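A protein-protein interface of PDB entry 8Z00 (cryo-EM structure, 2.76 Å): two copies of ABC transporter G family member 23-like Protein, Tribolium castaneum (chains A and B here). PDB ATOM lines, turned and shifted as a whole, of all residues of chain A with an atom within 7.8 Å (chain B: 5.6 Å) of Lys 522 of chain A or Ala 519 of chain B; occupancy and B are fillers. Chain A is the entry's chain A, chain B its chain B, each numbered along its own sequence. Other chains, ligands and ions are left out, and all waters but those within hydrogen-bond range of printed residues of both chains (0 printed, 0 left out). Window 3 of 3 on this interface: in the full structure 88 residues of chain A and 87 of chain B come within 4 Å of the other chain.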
ATOM      1  N   ARG A 517       6.229  18.088 -17.990  1.00  0.00           N
ATOM      2  CA  ARG A 517       5.082  17.293 -17.563  1.00  0.00           C
ATOM      3  C   ARG A 517       5.328  16.654 -16.203  1.00  0.00           C
ATOM      4  O   ARG A 517       4.432  16.623 -15.351  1.00  0.00           O
ATOM      5  CB  ARG A 517       4.765  16.230 -18.615  1.00  0.00           C
ATOM      6  CG  ARG A 517       4.075  14.987 -18.079  1.00  0.00           C
ATOM      7  CD  ARG A 517       3.759  14.010 -19.199  1.00  0.00           C
ATOM      8  NE  ARG A 517       2.667  13.109 -18.851  1.00  0.00           N
ATOM      9  CZ  ARG A 517       1.960  12.412 -19.731  1.00  0.00           C
ATOM     10  NH1 ARG A 517       2.199  12.494 -21.029  1.00  0.00           N
ATOM     11  NH2 ARG A 517       0.990  11.612 -19.297  1.00  0.00           N
ATOM     12  N   ALA A 519       7.379  17.754 -13.915  1.00  0.00           N
ATOM     13  CA  ALA A 519       7.665  18.764 -12.904  1.00  0.00           C
ATOM     14  C   ALA A 519       6.447  19.594 -12.531  1.00  0.00           C
ATOM     15  O   ALA A 519       6.509  20.350 -11.555  1.00  0.00           O
ATOM     16  CB  ALA A 519       8.786  19.695 -13.380  1.00  0.00           C
ATOM     17  N   LEU A 520       5.350  19.480 -13.278  1.00  0.00           N
ATOM     18  CA  LEU A 520       4.123  20.196 -12.959  1.00  0.00           C
ATOM     19  C   LEU A 520       3.155  19.330 -12.160  1.00  0.00           C
ATOM     20  O   LEU A 520       2.546  19.802 -11.195  1.00  0.00           O
ATOM     21  CB  LEU A 520       3.453  20.691 -14.244  1.00  0.00           C
ATOM     22  CG  LEU A 520       4.065  21.924 -14.907  1.00  0.00           C
ATOM     23  CD1 LEU A 520       3.618  22.030 -16.355  1.00  0.00           C
ATOM     24  CD2 LEU A 520       3.699  23.182 -14.138  1.00  0.00           C
ATOM     25  N   GLY A 521       3.005  18.077 -12.543  1.00  0.00           N
ATOM     26  CA  GLY A 521       2.101  17.164 -11.848  1.00  0.00           C
ATOM     27  C   GLY A 521       0.662  17.349 -12.312  1.00  0.00           C
ATOM     28  O   GLY A 521       0.371  17.199 -13.494  1.00  0.00           O
ATOM     29  N   LYS A 522      -0.227  17.672 -11.372  1.00  0.00           N
ATOM     30  CA  LYS A 522      -1.625  17.913 -11.705  1.00  0.00           C
ATOM     31  C   LYS A 522      -1.840  19.238 -12.423  1.00  0.00           C
ATOM     32  O   LYS A 522      -2.928  19.458 -12.966  1.00  0.00           O
ATOM     33  CB  LYS A 522      -2.481  17.873 -10.439  1.00  0.00           C
ATOM     34  CG  LYS A 522      -2.142  16.733  -9.496  1.00  0.00           C
ATOM     35  CD  LYS A 522      -1.672  17.260  -8.150  1.00  0.00           C
ATOM     36  CE  LYS A 522      -2.828  17.829  -7.345  1.00  0.00           C
ATOM     37  NZ  LYS A 522      -2.416  18.193  -5.962  1.00  0.00           N
ATOM     38  N   ASP A 523      -0.839  20.120 -12.439  1.00  0.00           N
ATOM     39  CA  ASP A 523      -0.946  21.428 -13.070  1.00  0.00           C
ATOM     40  C   ASP A 523      -0.319  21.451 -14.459  1.00  0.00           C
ATOM     41  O   ASP A 523       0.255  22.467 -14.865  1.00  0.00           O
ATOM     42  CB  ASP A 523      -0.306  22.496 -12.184  1.00  0.00           C
ATOM     43  CG  ASP A 523      -1.118  22.780 -10.937  1.00  0.00           C
ATOM     44  OD1 ASP A 523      -2.297  22.373 -10.890  1.00  0.00           O
ATOM     45  OD2 ASP A 523      -0.577  23.411 -10.004  1.00  0.00           O
ATOM     46  N   ALA A 524      -0.417  20.348 -15.196  1.00  0.00           N
ATOM     47  CA  ALA A 524       0.155  20.256 -16.532  1.00  0.00           C
ATOM     48  C   ALA A 524      -0.892  20.642 -17.570  1.00  0.00           C
ATOM     49  O   ALA A 524      -1.987  20.071 -17.600  1.00  0.00           O
ATOM     50  CB  ALA A 524       0.678  18.846 -16.800  1.00  0.00           C
ATOM     51  N   ASP A 525      -0.550  21.612 -18.413  1.00  0.00           N
ATOM     52  CA  ASP A 525      -1.457  22.074 -19.447  1.00  0.00           C
ATOM     53  C   ASP A 525      -1.563  21.038 -20.564  1.00  0.00           C
ATOM     54  O   ASP A 525      -0.687  20.183 -20.715  1.00  0.00           O
ATOM     55  CB  ASP A 525      -0.981  23.413 -20.003  1.00  0.00           C
ATOM     56  CG  ASP A 525       0.502  23.420 -20.310  1.00  0.00           C
ATOM     57  OD1 ASP A 525       1.306  23.578 -19.367  1.00  0.00           O
ATOM     58  OD2 ASP A 525       0.864  23.275 -21.496  1.00  0.00           O
ATOM     59  N   LEU A 529       1.019  17.938 -22.348  1.00  0.00           N
ATOM     60  CA  LEU A 529       0.504  16.577 -22.306  1.00  0.00           C
ATOM     61  C   LEU A 529       0.431  15.941 -23.685  1.00  0.00           C
ATOM     62  O   LEU A 529       0.358  14.711 -23.784  1.00  0.00           O
ATOM     63  CB  LEU A 529      -0.880  16.554 -21.653  1.00  0.00           C
ATOM     64  CG  LEU A 529      -0.923  16.610 -20.126  1.00  0.00           C
ATOM     65  CD1 LEU A 529      -2.348  16.449 -19.628  1.00  0.00           C
ATOM     66  CD2 LEU A 529      -0.017  15.554 -19.518  1.00  0.00           C
ATOM     67  N   LEU B 514      -4.515   6.339  -0.167  1.00  0.00           N
ATOM     68  CA  LEU B 514      -4.625   6.605  -1.599  1.00  0.00           C
ATOM     69  C   LEU B 514      -4.981   8.061  -1.869  1.00  0.00           C
ATOM     70  O   LEU B 514      -4.449   8.670  -2.803  1.00  0.00           O
ATOM     71  CB  LEU B 514      -5.656   5.673  -2.234  1.00  0.00           C
ATOM     72  CG  LEU B 514      -5.806   5.791  -3.752  1.00  0.00           C
ATOM     73  CD1 LEU B 514      -4.633   5.134  -4.457  1.00  0.00           C
ATOM     74  CD2 LEU B 514      -7.121   5.187  -4.216  1.00  0.00           C
ATOM     75  N   VAL B 515      -5.885   8.635  -1.071  1.00  0.00           N
ATOM     76  CA  VAL B 515      -6.254  10.036  -1.253  1.00  0.00           C
ATOM     77  C   VAL B 515      -5.049  10.938  -1.024  1.00  0.00           C
ATOM     78  O   VAL B 515      -4.806  11.882  -1.786  1.00  0.00           O
ATOM     79  CB  VAL B 515      -7.426  10.407  -0.326  1.00  0.00           C
ATOM     80  CG1 VAL B 515      -7.607  11.913  -0.274  1.00  0.00           C
ATOM     81  CG2 VAL B 515      -8.704   9.741  -0.799  1.00  0.00           C
ATOM     82  N   ALA B 516      -4.273  10.661   0.024  1.00  0.00           N
ATOM     83  CA  ALA B 516      -3.076  11.446   0.297  1.00  0.00           C
ATOM     84  C   ALA B 516      -1.979  11.200  -0.729  1.00  0.00           C
ATOM     85  O   ALA B 516      -1.154  12.089  -0.968  1.00  0.00           O
ATOM     86  CB  ALA B 516      -2.553  11.136   1.699  1.00  0.00           C
ATOM     87  N   ARG B 517      -1.941  10.009  -1.332  1.00  0.00           N
ATOM     88  CA  ARG B 517      -0.890   9.700  -2.297  1.00  0.00           C
ATOM     89  C   ARG B 517      -0.999  10.578  -3.537  1.00  0.00           C
ATOM     90  O   ARG B 517       0.011  11.090  -4.033  1.00  0.00           O
ATOM     91  CB  ARG B 517      -0.943   8.220  -2.673  1.00  0.00           C
ATOM     92  CG  ARG B 517      -0.374   7.894  -4.045  1.00  0.00           C
ATOM     93  CD  ARG B 517      -0.507   6.413  -4.354  1.00  0.00           C
ATOM     94  NE  ARG B 517       0.533   5.945  -5.263  1.00  0.00           N
ATOM     95  CZ  ARG B 517       1.181   4.796  -5.132  1.00  0.00           C
ATOM     96  NH1 ARG B 517       0.932   3.973  -4.129  1.00  0.00           N
ATOM     97  NH2 ARG B 517       2.104   4.465  -6.031  1.00  0.00           N
ATOM     98  N   MET B 518      -2.213  10.768  -4.053  1.00  0.00           N
ATOM     99  CA  MET B 518      -2.407  11.632  -5.210  1.00  0.00           C
ATOM    100  C   MET B 518      -2.352  13.113  -4.863  1.00  0.00           C
ATOM    101  O   MET B 518      -2.122  13.931  -5.758  1.00  0.00           O
ATOM    102  CB  MET B 518      -3.742  11.321  -5.895  1.00  0.00           C
ATOM    103  CG  MET B 518      -4.277   9.928  -5.629  1.00  0.00           C
ATOM    104  SD  MET B 518      -5.743   9.539  -6.604  1.00  0.00           S
ATOM    105  CE  MET B 518      -7.046   9.926  -5.438  1.00  0.00           C
ATOM    106  N   ALA B 519      -2.553  13.477  -3.597  1.00  0.00           N
ATOM    107  CA  ALA B 519      -2.503  14.871  -3.184  1.00  0.00           C
ATOM    108  C   ALA B 519      -1.096  15.351  -2.858  1.00  0.00           C
ATOM    109  O   ALA B 519      -0.868  16.564  -2.820  1.00  0.00           O
ATOM    110  CB  ALA B 519      -3.405  15.101  -1.966  1.00  0.00           C
ATOM    111  N   LEU B 520      -0.157  14.436  -2.622  1.00  0.00           N
ATOM    112  CA  LEU B 520       1.220  14.813  -2.337  1.00  0.00           C
ATOM    113  C   LEU B 520       2.108  14.778  -3.571  1.00  0.00           C
ATOM    114  O   LEU B 520       3.014  15.610  -3.695  1.00  0.00           O
ATOM    115  CB  LEU B 520       1.806  13.894  -1.261  1.00  0.00           C
ATOM    116  CG  LEU B 520       2.030  14.522   0.114  1.00  0.00           C
ATOM    117  CD1 LEU B 520       0.771  15.229   0.593  1.00  0.00           C
ATOM    118  CD2 LEU B 520       2.471  13.469   1.117  1.00  0.00           C
ATOM    119  N   GLY B 521       1.871  13.839  -4.483  1.00  0.00           N
ATOM    120  CA  GLY B 521       2.668  13.746  -5.690  1.00  0.00           C
ATOM    121  C   GLY B 521       3.993  13.046  -5.475  1.00  0.00           C
ATOM    122  O   GLY B 521       4.029  11.883  -5.062  1.00  0.00           O
ATOM    123  N   LEU B 574      -4.620  13.156 -17.796  1.00  0.00           N
ATOM    124  CA  LEU B 574      -3.609  13.186 -16.747  1.00  0.00           C
ATOM    125  C   LEU B 574      -3.277  11.794 -16.223  1.00  0.00           C
ATOM    126  O   LEU B 574      -2.222  11.614 -15.606  1.00  0.00           O
ATOM    127  CB  LEU B 574      -4.075  14.075 -15.594  1.00  0.00           C
ATOM    128  CG  LEU B 574      -4.052  15.583 -15.844  1.00  0.00           C
ATOM    129  CD1 LEU B 574      -4.972  16.295 -14.868  1.00  0.00           C
ATOM    130  CD2 LEU B 574      -2.635  16.121 -15.738  1.00  0.00           C
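Among the printed residues, pairs that only touch across the chains: Lys 522 of chain A with Ala 519 of chain B, Gly 521 of chain A with Leu 574 of chain B and Leu 529 of chain A with Leu 574 of chain B.
Printed residues of chain B within 4 Å of Gly 521 of chain A: Leu 574.
Lys 522 of chain A touches one residue of chain B.
Printed residues of chain B within 4 Å of Leu 529 of chain A: Leu 574 (3.9 Å).
Val 515 of chain B touches none of the printed residues of chain A.
Of the printed residues of chain A, Ala 519 of chain B touches Lys 522 (3.9 Å).
Printed residues of chain A within 4 Å of Leu 574 of chain B: Gly 521 and Leu 529.
The nearest printed residue of chain A that does not touch Ala 519 of chain B is Gly 521 of chain A (9.5 Å).
The nearest printed residue of chain B that does not touch Leu 529 of chain A is Met 518 of chain B (14.0 Å).
Of the 9 printed residues of chain A, 3 touch a printed residue of chain B.
Hydrophobic or aromatic side chains of chain B that line the printed part of chain A: Leu 574.
Among the printed residues, no Asp or Glu carboxylate lies within 4 Å of a Lys or Arg side-chain nitrogen of the other chain.
4 positions are printed for both chains.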
